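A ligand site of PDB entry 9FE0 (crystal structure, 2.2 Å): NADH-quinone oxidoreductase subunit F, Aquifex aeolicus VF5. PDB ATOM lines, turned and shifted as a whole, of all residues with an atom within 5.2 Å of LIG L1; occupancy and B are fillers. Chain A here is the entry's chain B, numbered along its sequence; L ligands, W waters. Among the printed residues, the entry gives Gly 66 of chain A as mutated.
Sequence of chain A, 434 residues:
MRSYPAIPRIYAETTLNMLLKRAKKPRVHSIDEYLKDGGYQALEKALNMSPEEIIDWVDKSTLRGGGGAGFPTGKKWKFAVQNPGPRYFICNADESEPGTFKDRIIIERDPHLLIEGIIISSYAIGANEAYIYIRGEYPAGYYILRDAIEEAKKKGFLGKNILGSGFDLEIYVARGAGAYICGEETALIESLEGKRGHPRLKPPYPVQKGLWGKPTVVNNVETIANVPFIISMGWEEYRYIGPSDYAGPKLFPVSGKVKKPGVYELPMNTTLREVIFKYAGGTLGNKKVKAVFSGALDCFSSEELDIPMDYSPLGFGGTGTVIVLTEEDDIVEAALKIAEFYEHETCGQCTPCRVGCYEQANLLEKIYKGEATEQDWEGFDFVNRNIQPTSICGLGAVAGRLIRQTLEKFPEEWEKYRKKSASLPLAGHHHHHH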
ATOM      1  N   GLY A  65     -20.068  14.730 -13.546  1.00  0.00           N
ATOM      2  CA  GLY A  65     -19.963  15.008 -12.129  1.00  0.00           C
ATOM      3  C   GLY A  65     -21.286  15.508 -11.571  1.00  0.00           C
ATOM      4  O   GLY A  65     -21.947  16.351 -12.178  1.00  0.00           O
ATOM      5  N   GLY A  66     -21.693  14.951 -10.431  1.00  0.00           N
ATOM      6  CA  GLY A  66     -22.936  15.337  -9.784  1.00  0.00           C
ATOM      7  C   GLY A  66     -22.681  16.347  -8.661  1.00  0.00           C
ATOM      8  O   GLY A  66     -23.591  16.659  -7.905  1.00  0.00           O
ATOM      9  N   GLY A  67     -21.437  16.832  -8.579  1.00  0.00           N
ATOM     10  CA  GLY A  67     -21.048  17.786  -7.553  1.00  0.00           C
ATOM     11  C   GLY A  67     -21.456  19.212  -7.918  1.00  0.00           C
ATOM     12  O   GLY A  67     -21.471  20.078  -7.049  1.00  0.00           O
ATOM     13  N   GLY A  68     -21.744  19.451  -9.207  1.00  0.00           N
ATOM     14  CA  GLY A  68     -22.281  20.736  -9.627  1.00  0.00           C
ATOM     15  C   GLY A  68     -21.706  21.228 -10.956  1.00  0.00           C
ATOM     16  O   GLY A  68     -22.364  21.966 -11.675  1.00  0.00           O
ATOM     17  N   ALA A  69     -20.472  20.825 -11.272  1.00  0.00           N
ATOM     18  CA  ALA A  69     -19.781  21.359 -12.427  1.00  0.00           C
ATOM     19  C   ALA A  69     -20.030  20.497 -13.665  1.00  0.00           C
ATOM     20  O   ALA A  69     -19.777  20.943 -14.786  1.00  0.00           O
ATOM     21  CB  ALA A  69     -18.305  21.494 -12.134  1.00  0.00           C
ATOM     22  N   GLY A  70     -20.492  19.261 -13.464  1.00  0.00           N
ATOM     23  CA  GLY A  70     -20.888  18.385 -14.551  1.00  0.00           C
ATOM     24  C   GLY A  70     -19.712  17.969 -15.431  1.00  0.00           C
ATOM     25  O   GLY A  70     -19.907  17.707 -16.625  1.00  0.00           O
ATOM     26  N   PHE A  71     -18.517  17.875 -14.848  1.00  0.00           N
ATOM     27  CA  PHE A  71     -17.338  17.493 -15.624  1.00  0.00           C
ATOM     28  C   PHE A  71     -17.387  15.993 -15.937  1.00  0.00           C
ATOM     29  O   PHE A  71     -17.730  15.175 -15.077  1.00  0.00           O
ATOM     30  CB  PHE A  71     -16.047  17.835 -14.874  1.00  0.00           C
ATOM     31  CG  PHE A  71     -14.810  17.752 -15.738  1.00  0.00           C
ATOM     32  CD1 PHE A  71     -14.402  18.858 -16.497  1.00  0.00           C
ATOM     33  CD2 PHE A  71     -14.050  16.598 -15.800  1.00  0.00           C
ATOM     34  CE1 PHE A  71     -13.276  18.775 -17.310  1.00  0.00           C
ATOM     35  CE2 PHE A  71     -12.913  16.530 -16.591  1.00  0.00           C
ATOM     36  CZ  PHE A  71     -12.538  17.619 -17.351  1.00  0.00           C
ATOM     37  N   THR A  73     -16.724  12.301 -16.062  1.00  0.00           N
ATOM     38  CA  THR A  73     -16.063  11.528 -15.015  1.00  0.00           C
ATOM     39  C   THR A  73     -14.936  10.682 -15.609  1.00  0.00           C
ATOM     40  O   THR A  73     -13.842  10.661 -15.067  1.00  0.00           O
ATOM     41  CB  THR A  73     -17.083  10.648 -14.307  1.00  0.00           C
ATOM     42  OG1 THR A  73     -18.076  11.463 -13.697  1.00  0.00           O
ATOM     43  CG2 THR A  73     -16.425   9.805 -13.237  1.00  0.00           C
ATOM     44  N   LYS A  76     -11.958  12.684 -16.393  1.00  0.00           N
ATOM     45  CA  LYS A  76     -11.238  13.039 -15.194  1.00  0.00           C
ATOM     46  C   LYS A  76     -10.282  11.911 -14.801  1.00  0.00           C
ATOM     47  O   LYS A  76      -9.114  12.152 -14.504  1.00  0.00           O
ATOM     48  CB  LYS A  76     -12.186  13.355 -14.035  1.00  0.00           C
ATOM     49  CG  LYS A  76     -11.504  14.034 -12.851  1.00  0.00           C
ATOM     50  CD  LYS A  76     -12.376  14.253 -11.622  1.00  0.00           C
ATOM     51  CE  LYS A  76     -13.575  15.130 -11.829  1.00  0.00           C
ATOM     52  NZ  LYS A  76     -14.194  15.548 -10.561  1.00  0.00           N
ATOM     53  N   ASN A  92     -16.321  13.144  -2.213  1.00  0.00           N
ATOM     54  CA  ASN A  92     -16.705  14.438  -1.667  1.00  0.00           C
ATOM     55  C   ASN A  92     -18.135  14.343  -1.142  1.00  0.00           C
ATOM     56  O   ASN A  92     -19.097  14.404  -1.912  1.00  0.00           O
ATOM     57  CB  ASN A  92     -16.566  15.532  -2.726  1.00  0.00           C
ATOM     58  CG  ASN A  92     -16.684  16.953  -2.189  1.00  0.00           C
ATOM     59  OD1 ASN A  92     -17.181  17.179  -1.084  1.00  0.00           O
ATOM     60  ND2 ASN A  92     -16.257  17.914  -2.994  1.00  0.00           N
ATOM     61  N   ASP A  94     -19.247  16.583   1.294  1.00  0.00           N
ATOM     62  CA  ASP A  94     -19.330  17.809   2.081  1.00  0.00           C
ATOM     63  C   ASP A  94     -20.682  18.492   1.915  1.00  0.00           C
ATOM     64  O   ASP A  94     -21.041  19.302   2.761  1.00  0.00           O
ATOM     65  CB  ASP A  94     -18.215  18.788   1.775  1.00  0.00           C
ATOM     66  CG  ASP A  94     -18.060  19.873   2.837  1.00  0.00           C
ATOM     67  OD1 ASP A  94     -17.758  19.511   3.993  1.00  0.00           O
ATOM     68  OD2 ASP A  94     -18.333  21.041   2.534  1.00  0.00           O
ATOM     69  N   GLU A  95     -21.436  18.141   0.858  1.00  0.00           N
ATOM     70  CA  GLU A  95     -22.770  18.666   0.554  1.00  0.00           C
ATOM     71  C   GLU A  95     -23.244  19.747   1.530  1.00  0.00           C
ATOM     72  O   GLU A  95     -23.882  19.427   2.547  1.00  0.00           O
ATOM     73  CB  GLU A  95     -23.752  17.495   0.526  1.00  0.00           C
ATOM     74  CG  GLU A  95     -25.186  17.924   0.243  1.00  0.00           C
ATOM     75  CD  GLU A  95     -26.133  16.779   0.006  1.00  0.00           C
ATOM     76  OE1 GLU A  95     -26.550  16.060   0.978  1.00  0.00           O
ATOM     77  OE2 GLU A  95     -26.462  16.628  -1.195  1.00  0.00           O
ATOM     78  N   SER A  96     -22.965  21.020   1.203  1.00  0.00           N
ATOM     79  CA  SER A  96     -23.340  22.125   2.081  1.00  0.00           C
ATOM     80  C   SER A  96     -23.989  23.309   1.360  1.00  0.00           C
ATOM     81  O   SER A  96     -24.333  24.291   2.023  1.00  0.00           O
ATOM     82  CB  SER A  96     -22.160  22.568   2.914  1.00  0.00           C
ATOM     83  OG  SER A  96     -21.948  21.666   3.991  1.00  0.00           O
ATOM     84  N   ASP A 103     -27.217  13.948  -1.620  1.00  0.00           N
ATOM     85  CA  ASP A 103     -26.161  12.974  -1.372  1.00  0.00           C
ATOM     86  C   ASP A 103     -26.414  12.220  -0.064  1.00  0.00           C
ATOM     87  O   ASP A 103     -26.096  11.034   0.046  1.00  0.00           O
ATOM     88  CB  ASP A 103     -24.797  13.637  -1.322  1.00  0.00           C
ATOM     89  CG  ASP A 103     -24.327  14.345  -2.597  1.00  0.00           C
ATOM     90  OD1 ASP A 103     -24.931  14.118  -3.673  1.00  0.00           O
ATOM     91  OD2 ASP A 103     -23.358  15.134  -2.490  1.00  0.00           O
ATOM     92  N   TYR A 180     -18.263  25.565   4.654  1.00  0.00           N
ATOM     93  CA  TYR A 180     -18.746  25.323   3.294  1.00  0.00           C
ATOM     94  C   TYR A 180     -17.586  25.157   2.310  1.00  0.00           C
ATOM     95  O   TYR A 180     -17.675  24.357   1.379  1.00  0.00           O
ATOM     96  CB  TYR A 180     -19.638  26.486   2.874  1.00  0.00           C
ATOM     97  CG  TYR A 180     -20.028  26.629   1.405  1.00  0.00           C
ATOM     98  CD1 TYR A 180     -20.965  25.791   0.819  1.00  0.00           C
ATOM     99  CD2 TYR A 180     -19.517  27.655   0.626  1.00  0.00           C
ATOM    100  CE1 TYR A 180     -21.365  25.958  -0.498  1.00  0.00           C
ATOM    101  CE2 TYR A 180     -19.898  27.836  -0.699  1.00  0.00           C
ATOM    102  CZ  TYR A 180     -20.831  26.982  -1.266  1.00  0.00           C
ATOM    103  OH  TYR A 180     -21.190  27.160  -2.572  1.00  0.00           O
ATOM    104  N   ILE A 181     -16.510  25.920   2.525  1.00  0.00           N
ATOM    105  CA  ILE A 181     -15.409  25.993   1.568  1.00  0.00           C
ATOM    106  C   ILE A 181     -14.691  24.648   1.456  1.00  0.00           C
ATOM    107  O   ILE A 181     -14.131  24.322   0.410  1.00  0.00           O
ATOM    108  CB  ILE A 181     -14.424  27.126   1.954  1.00  0.00           C
ATOM    109  CG1 ILE A 181     -13.488  27.462   0.805  1.00  0.00           C
ATOM    110  CG2 ILE A 181     -13.662  26.790   3.238  1.00  0.00           C
ATOM    111  CD1 ILE A 181     -14.193  27.780  -0.502  1.00  0.00           C
ATOM    112  N   GLY A 183     -15.862  21.999   0.907  1.00  0.00           N
ATOM    113  CA  GLY A 183     -16.439  21.252  -0.206  1.00  0.00           C
ATOM    114  C   GLY A 183     -15.681  21.476  -1.516  1.00  0.00           C
ATOM    115  O   GLY A 183     -15.745  20.636  -2.421  1.00  0.00           O
ATOM    116  N   GLU A 184     -14.997  22.623  -1.618  1.00  0.00           N
ATOM    117  CA  GLU A 184     -14.135  22.910  -2.771  1.00  0.00           C
ATOM    118  C   GLU A 184     -12.993  21.909  -2.729  1.00  0.00           C
ATOM    119  O   GLU A 184     -12.380  21.705  -1.680  1.00  0.00           O
ATOM    120  CB  GLU A 184     -13.703  24.375  -2.787  1.00  0.00           C
ATOM    121  CG  GLU A 184     -13.214  24.863  -4.157  1.00  0.00           C
ATOM    122  CD  GLU A 184     -11.785  24.528  -4.537  1.00  0.00           C
ATOM    123  OE1 GLU A 184     -10.990  24.158  -3.659  1.00  0.00           O
ATOM    124  OE2 GLU A 184     -11.458  24.606  -5.749  1.00  0.00           O
ATOM    125  N   GLU A 185     -12.739  21.233  -3.851  1.00  0.00           N
ATOM    126  CA  GLU A 185     -11.908  20.034  -3.867  1.00  0.00           C
ATOM    127  C   GLU A 185     -10.503  20.298  -3.317  1.00  0.00           C
ATOM    128  O   GLU A 185      -9.960  19.424  -2.652  1.00  0.00           O
ATOM    129  CB  GLU A 185     -11.888  19.404  -5.253  1.00  0.00           C
ATOM    130  CG  GLU A 185     -11.289  20.296  -6.339  1.00  0.00           C
ATOM    131  CD  GLU A 185     -11.250  19.678  -7.724  1.00  0.00           C
ATOM    132  OE1 GLU A 185     -11.591  18.480  -7.891  1.00  0.00           O
ATOM    133  OE2 GLU A 185     -10.846  20.410  -8.644  1.00  0.00           O
ATOM    134  N   LYS A 202      -5.857  26.403  -9.153  1.00  0.00           N
ATOM    135  CA  LYS A 202      -5.940  25.403 -10.196  1.00  0.00           C
ATOM    136  C   LYS A 202      -5.723  26.100 -11.541  1.00  0.00           C
ATOM    137  O   LYS A 202      -6.369  27.106 -11.778  1.00  0.00           O
ATOM    138  CB  LYS A 202      -7.334  24.768 -10.233  1.00  0.00           C
ATOM    139  CG  LYS A 202      -7.818  24.134  -8.929  1.00  0.00           C
ATOM    140  CD  LYS A 202      -9.313  24.264  -8.661  1.00  0.00           C
ATOM    141  CE  LYS A 202     -10.205  23.531  -9.618  1.00  0.00           C
ATOM    142  NZ  LYS A 202     -11.523  23.237  -9.015  1.00  0.00           N
ATOM    143  N   VAL A 218     -11.034  13.591  -7.139  1.00  0.00           N
ATOM    144  CA  VAL A 218     -12.147  13.939  -6.287  1.00  0.00           C
ATOM    145  C   VAL A 218     -13.429  13.782  -7.088  1.00  0.00           C
ATOM    146  O   VAL A 218     -13.579  14.383  -8.158  1.00  0.00           O
ATOM    147  CB  VAL A 218     -12.035  15.379  -5.739  1.00  0.00           C
ATOM    148  CG1 VAL A 218     -13.152  15.682  -4.761  1.00  0.00           C
ATOM    149  CG2 VAL A 218     -10.683  15.638  -5.079  1.00  0.00           C
ATOM    150  N   ASN A 219     -14.355  12.950  -6.576  1.00  0.00           N
ATOM    151  CA  ASN A 219     -15.685  12.842  -7.140  1.00  0.00           C
ATOM    152  C   ASN A 219     -16.750  13.002  -6.067  1.00  0.00           C
ATOM    153  O   ASN A 219     -16.539  12.680  -4.897  1.00  0.00           O
ATOM    154  CB  ASN A 219     -15.919  11.514  -7.875  1.00  0.00           C
ATOM    155  CG  ASN A 219     -15.465  11.577  -9.301  1.00  0.00           C
ATOM    156  OD1 ASN A 219     -15.865  12.473 -10.065  1.00  0.00           O
ATOM    157  ND2 ASN A 219     -14.571  10.678  -9.658  1.00  0.00           N
ATOM    158  N   ASN A 220     -17.924  13.463  -6.520  1.00  0.00           N
ATOM    159  CA  ASN A 220     -19.094  13.650  -5.685  1.00  0.00           C
ATOM    160  C   ASN A 220     -19.768  12.294  -5.404  1.00  0.00           C
ATOM    161  O   ASN A 220     -19.717  11.405  -6.245  1.00  0.00           O
ATOM    162  CB  ASN A 220     -20.030  14.647  -6.374  1.00  0.00           C
ATOM    163  CG  ASN A 220     -21.338  14.783  -5.633  1.00  0.00           C
ATOM    164  OD1 ASN A 220     -21.396  15.361  -4.534  1.00  0.00           O
ATOM    165  ND2 ASN A 220     -22.394  14.243  -6.216  1.00  0.00           N
ATOM    166  N   VAL A 221     -20.384  12.174  -4.205  1.00  0.00           N
ATOM    167  CA  VAL A 221     -21.130  11.014  -3.741  1.00  0.00           C
ATOM    168  C   VAL A 221     -22.060  10.454  -4.820  1.00  0.00           C
ATOM    169  O   VAL A 221     -22.075   9.249  -5.041  1.00  0.00           O
ATOM    170  CB  VAL A 221     -21.972  11.364  -2.488  1.00  0.00           C
ATOM    171  CG1 VAL A 221     -23.077  10.346  -2.207  1.00  0.00           C
ATOM    172  CG2 VAL A 221     -21.109  11.542  -1.259  1.00  0.00           C
ATOM    173  N   THR A 223     -22.044  10.970  -8.103  1.00  0.00           N
ATOM    174  CA  THR A 223     -21.237  10.499  -9.217  1.00  0.00           C
ATOM    175  C   THR A 223     -20.828   9.051  -8.976  1.00  0.00           C
ATOM    176  O   THR A 223     -20.986   8.203  -9.851  1.00  0.00           O
ATOM    177  CB  THR A 223     -19.979  11.349  -9.398  1.00  0.00           C
ATOM    178  OG1 THR A 223     -20.310  12.716  -9.176  1.00  0.00           O
ATOM    179  CG2 THR A 223     -19.359  11.150 -10.772  1.00  0.00           C
ATOM    180  N   CYS A 393     -10.953  30.570  -6.534  1.00  0.00           N
ATOM    181  CA  CYS A 393     -11.892  29.450  -6.517  1.00  0.00           C
ATOM    182  C   CYS A 393     -13.286  29.954  -6.843  1.00  0.00           C
ATOM    183  O   CYS A 393     -13.513  31.156  -6.942  1.00  0.00           O
ATOM    184  CB  CYS A 393     -11.850  28.665  -5.194  1.00  0.00           C
ATOM    185  SG  CYS A 393     -13.023  29.201  -3.919  1.00  0.00           S
ATOM    186  N   GLY A 394     -14.218  29.010  -6.998  1.00  0.00           N
ATOM    187  CA  GLY A 394     -15.529  29.284  -7.570  1.00  0.00           C
ATOM    188  C   GLY A 394     -16.466  30.055  -6.623  1.00  0.00           C
ATOM    189  O   GLY A 394     -17.457  30.599  -7.099  1.00  0.00           O
ATOM    190  N   LEU A 395     -16.177  30.102  -5.323  1.00  0.00           N
ATOM    191  CA  LEU A 395     -17.040  30.844  -4.400  1.00  0.00           C
ATOM    192  C   LEU A 395     -16.984  32.319  -4.774  1.00  0.00           C
ATOM    193  O   LEU A 395     -18.023  32.980  -4.894  1.00  0.00           O
ATOM    194  CB  LEU A 395     -16.624  30.606  -2.941  1.00  0.00           C
ATOM    195  CG  LEU A 395     -17.557  31.164  -1.857  1.00  0.00           C
ATOM    196  CD1 LEU A 395     -17.326  30.411  -0.542  1.00  0.00           C
ATOM    197  CD2 LEU A 395     -17.371  32.652  -1.626  1.00  0.00           C
HETATM  198  C1  LIG L   1     -17.723  22.675  -4.547  1.00  0.00           C
HETATM  199  N1  LIG L   1     -17.899  21.362  -5.060  1.00  0.00           N
HETATM  200  C2  LIG L   1     -18.553  20.429  -4.280  1.00  0.00           C
HETATM  201  N2  LIG L   1     -18.665  19.143  -4.751  1.00  0.00           N
HETATM  202  C3  LIG L   1     -19.181  18.112  -4.003  1.00  0.00           C
HETATM  203  O1  LIG L   1     -19.143  16.939  -4.382  1.00  0.00           O
HETATM  204  N3  LIG L   1     -19.706  18.458  -2.784  1.00  0.00           N
HETATM  205  C4  LIG L   1     -19.675  19.709  -2.206  1.00  0.00           C
HETATM  206  O2  LIG L   1     -20.141  19.845  -1.071  1.00  0.00           O
HETATM  207  C5  LIG L   1     -19.049  20.720  -3.027  1.00  0.00           C
HETATM  208  N4  LIG L   1     -18.872  21.978  -2.540  1.00  0.00           N
HETATM  209  C6  LIG L   1     -18.201  22.954  -3.265  1.00  0.00           C
HETATM  210  C7  LIG L   1     -18.022  24.228  -2.726  1.00  0.00           C
HETATM  211  C8  LIG L   1     -17.381  25.232  -3.447  1.00  0.00           C
HETATM  212  C9  LIG L   1     -17.174  26.587  -2.829  1.00  0.00           C
HETATM  213  C10 LIG L   1     -16.908  24.948  -4.750  1.00  0.00           C
HETATM  214  C11 LIG L   1     -16.279  26.029  -5.593  1.00  0.00           C
HETATM  215  C12 LIG L   1     -17.073  23.676  -5.278  1.00  0.00           C
HETATM  216  C13 LIG L   1     -17.345  20.997  -6.372  1.00  0.00           C
HETATM  217  C14 LIG L   1     -15.987  20.339  -6.143  1.00  0.00           C
HETATM  218  O3  LIG L   1     -14.985  21.356  -6.071  1.00  0.00           O
HETATM  219  C15 LIG L   1     -15.689  19.376  -7.296  1.00  0.00           C
HETATM  220  O4  LIG L   1     -16.046  19.996  -8.523  1.00  0.00           O
HETATM  221  C16 LIG L   1     -16.422  18.040  -7.203  1.00  0.00           C
HETATM  222  O5  LIG L   1     -16.386  17.489  -5.875  1.00  0.00           O
HETATM  223  C17 LIG L   1     -15.881  17.064  -8.229  1.00  0.00           C
HETATM  224  O6  LIG L   1     -16.729  15.886  -8.259  1.00  0.00           O
HETATM  225  P1  LIG L   1     -17.651  15.550  -9.545  1.00  0.00           P
HETATM  226  O7  LIG L   1     -16.827  15.800 -10.793  1.00  0.00           O
HETATM  227  O8  LIG L   1     -17.991  14.083  -9.349  1.00  0.00           O
HETATM  228  O9  LIG L   1     -18.857  16.457  -9.436  1.00  0.00           O
HETATM  229  P1  LG2 L   2     -14.581  23.193 -11.971  1.00  0.00           P
HETATM  230  O1  LG2 L   2     -15.300  23.423 -13.258  1.00  0.00           O
HETATM  231  O2  LG2 L   2     -13.422  24.072 -11.664  1.00  0.00           O
HETATM  232  O3  LG2 L   2     -14.075  21.671 -11.889  1.00  0.00           O
HETATM  233  C1  LG2 L   2     -15.015  20.581 -11.808  1.00  0.00           C
HETATM  234  C2  LG2 L   2     -14.269  19.278 -11.695  1.00  0.00           C
HETATM  235  O4  LG2 L   2     -13.606  18.997 -12.958  1.00  0.00           O
HETATM  236  C3  LG2 L   2     -13.158  19.241 -10.642  1.00  0.00           C
HETATM  237  O5  LG2 L   2     -13.022  17.959 -10.048  1.00  0.00           O
HETATM  238  C4  LG2 L   2     -11.919  19.625 -11.456  1.00  0.00           C
HETATM  239  O6  LG2 L   2     -10.743  19.147 -10.844  1.00  0.00           O
HETATM  240  C5  LG2 L   2     -12.210  18.923 -12.777  1.00  0.00           C
HETATM  241  N1  LG2 L   2     -11.547  19.531 -13.934  1.00  0.00           N
HETATM  242  C6  LG2 L   2     -11.958  20.624 -14.636  1.00  0.00           C
HETATM  243  N2  LG2 L   2     -11.173  20.939 -15.635  1.00  0.00           N
HETATM  244  C7  LG2 L   2     -10.168  19.981 -15.587  1.00  0.00           C
HETATM  245  C8  LG2 L   2      -9.016  19.776 -16.373  1.00  0.00           C
HETATM  246  N3  LG2 L   2      -8.678  20.546 -17.409  1.00  0.00           N
HETATM  247  N4  LG2 L   2      -8.208  18.740 -16.050  1.00  0.00           N
HETATM  248  C9  LG2 L   2      -8.555  17.975 -15.013  1.00  0.00           C
HETATM  249  N5  LG2 L   2      -9.604  18.072 -14.199  1.00  0.00           N
HETATM  250  C10 LG2 L   2     -10.381  19.104 -14.543  1.00  0.00           C
HETATM  251  O7  LG2 L   2     -15.624  23.317 -10.782  1.00  0.00           O
HETATM  252  P2  LG2 L   2     -15.402  23.559  -9.208  1.00  0.00           P
HETATM  253  O8  LG2 L   2     -14.881  24.953  -9.021  1.00  0.00           O
HETATM  254  O9  LG2 L   2     -14.590  22.436  -8.633  1.00  0.00           O
HETATM  255  O10 LG2 L   2     -16.904  23.456  -8.664  1.00  0.00           O
HETATM  256  C11 LG2 L   2     -17.901  24.500  -8.803  1.00  0.00           C
HETATM  257  C12 LG2 L   2     -19.281  23.901  -8.595  1.00  0.00           C
HETATM  258  O11 LG2 L   2     -19.433  23.442  -7.235  1.00  0.00           O
HETATM  259  C13 LG2 L   2     -20.477  24.848  -8.824  1.00  0.00           C
HETATM  260  O12 LG2 L   2     -21.020  24.656 -10.117  1.00  0.00           O
HETATM  261  C14 LG2 L   2     -21.487  24.487  -7.708  1.00  0.00           C
HETATM  262  O13 LG2 L   2     -22.747  24.037  -8.148  1.00  0.00           O
HETATM  263  C15 LG2 L   2     -20.830  23.280  -7.019  1.00  0.00           C
HETATM  264  N6  LG2 L   2     -21.128  23.184  -5.569  1.00  0.00           N
HETATM  265  C16 LG2 L   2     -21.778  22.068  -5.061  1.00  0.00           C
HETATM  266  C17 LG2 L   2     -22.058  21.994  -3.698  1.00  0.00           C
HETATM  267  C18 LG2 L   2     -22.742  20.784  -3.099  1.00  0.00           C
HETATM  268  O14 LG2 L   2     -23.038  20.782  -1.890  1.00  0.00           O
HETATM  269  N7  LG2 L   2     -22.989  19.747  -3.884  1.00  0.00           N
HETATM  270  C19 LG2 L   2     -21.680  23.033  -2.864  1.00  0.00           C
HETATM  271  C20 LG2 L   2     -21.045  24.146  -3.383  1.00  0.00           C
HETATM  272  C21 LG2 L   2     -20.778  24.215  -4.736  1.00  0.00           C
HETATM  273  O   HOH W   1     -19.732  22.440   0.515  1.00  0.00           O
HETATM  274  O   HOH W   2     -16.889  13.893 -12.789  1.00  0.00           O
HETATM  275  O   HOH W   3     -18.572  19.163  -9.688  1.00  0.00           O
HETATM  276  O   HOH W   4     -21.033  16.314  -1.567  1.00  0.00           O
HETATM  277  O   HOH W   5     -17.734  18.028 -12.263  1.00  0.00           O
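NZ of Lys 76 is in salt-bridge range of O7 of LIG L1 (2.7 Å). The side-chain hydroxyl (OG1) of Thr 223 is in hydrogen-bond range of an oxygen (O8) of LIG L1, at 2.7 Å. An oxygen (O9) of LIG L1 is in hydrogen-bond range of the backbone NH of Gly 67, 2.7 Å away. N of Asn 220 lies within hydrogen-bond range of O8 of LIG L1, at 2.9 Å. The side-chain amide oxygen of Asn 220 sits close to an oxygen (O1) of LIG L1 (2.8 Å). An oxygen (O8) of LIG L1 lies close to the side-chain amide oxygen (OD1) of Asn 219, 2.8 Å away. An oxygen (O2) of LIG L1 sits at hydrogen-bond distance from the backbone NH (N) of Glu 95, at 2.9 Å. An oxygen (O5) of LIG L1 lies within hydrogen-bond range of the side-chain amide nitrogen of Asn 92. The backbone NH of Glu 185 sits at hydrogen-bond distance from an oxygen (O3) of LIG L1, 3.2 Å away. N of Gly 66 lies within hydrogen-bond range of O9 of LIG L1. A nitrogen (N4) of LIG L1 lies close to the backbone carbonyl oxygen of Gly 183. An oxygen (O5) of LG2 L2 sits at hydrogen-bond distance from the side-chain amino group (NZ) of Lys 76 (2.7 Å). An oxygen (O6) of LG2 L2 is in hydrogen-bond range of the side-chain carboxylate of Glu 185 (2.5 Å). An oxygen (O14) of LG2 L2 sits at hydrogen-bond distance from the backbone NH of Ser 96 (3.1 Å). The backbone carbonyl oxygen of Gly 68 sits at hydrogen-bond distance from an oxygen (O12) of LG2 L2. The side-chain amino group (NZ) of Lys 202 lies within salt-bridge range of an oxygen (O9) of LG2 L2 (3.2 Å).
O9 of LG2 L2 sits at hydrogen-bond distance from O3 of LIG L1.
The side-chain hydroxyl (OG1) of Thr 223 sits close to the backbone carbonyl oxygen (O) of Asn 220. The backbone NH of Gly 66 lies within hydrogen-bond range of the side-chain hydroxyl of Thr 223, at 2.9 Å. OD1 of Asn 220 sits close to OD2 of Asp 103, at 2.8 Å. The side-chain amide nitrogen (ND2) of Asn 92 sits at hydrogen-bond distance from the backbone carbonyl oxygen (O) of Gly 183. The side-chain carboxylate (OE2) of Glu 185 lies within salt-bridge range of the side-chain amino group (NZ) of Lys 202 (2.9 Å). OD2 of Asp 94 lies within hydrogen-bond range of N of Gly 183, at 3.1 Å. The backbone carbonyl oxygen of Asp 94 lies within hydrogen-bond range of the side-chain hydroxyl of Ser 96 (2.8 Å). OE2 of Glu 184 lies within salt-bridge range of NZ of Lys 202 (3.5 Å).
The backbone carbonyl oxygen of Val 218 lies close to an oxygen (O6) of LIG L1 (3.5 Å). Gly 65 touches LIG L1. Asp 94 touches LIG L1. Ser 96 touches LIG L1 (N to O2, 3.8 Å). Tyr 180 touches LIG L1. Ile 181 touches LIG L1 (CD1 to C9, 3.97 Å). CG of Glu 184 touches C11 of LIG L1, at 3.6 Å. Gly 394 touches LIG L1 (CA to C11, 3.9 Å). Hydrophobic or aromatic side chains within 4 Å of LIG L1: Tyr 180, Ile 181 and Val 218. The nearest printed residue that does not touch LIG L1 is Leu 395 (4.1 Å).
Water W3 lies within hydrogen-bond range of an oxygen (O9) of LIG L1, the backbone NH (N) of Ala 69 and the backbone NH (N) of Gly 68. Water W2 lies within hydrogen-bond range of the backbone carbonyl oxygen of Phe 71 (2.8 Å), an oxygen (O7) of LIG L1 (2.8 Å), the side-chain hydroxyl of Thr 73 (2.9 Å), the side-chain amide oxygen of Asn 219 (3.2 Å) and the backbone NH of Gly 65 (3.4 Å). Water W5 lies within hydrogen-bond range of N of Phe 71 (2.7 Å), O7 of LIG L1 (2.8 Å) and N of Gly 70 (3.3 Å).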
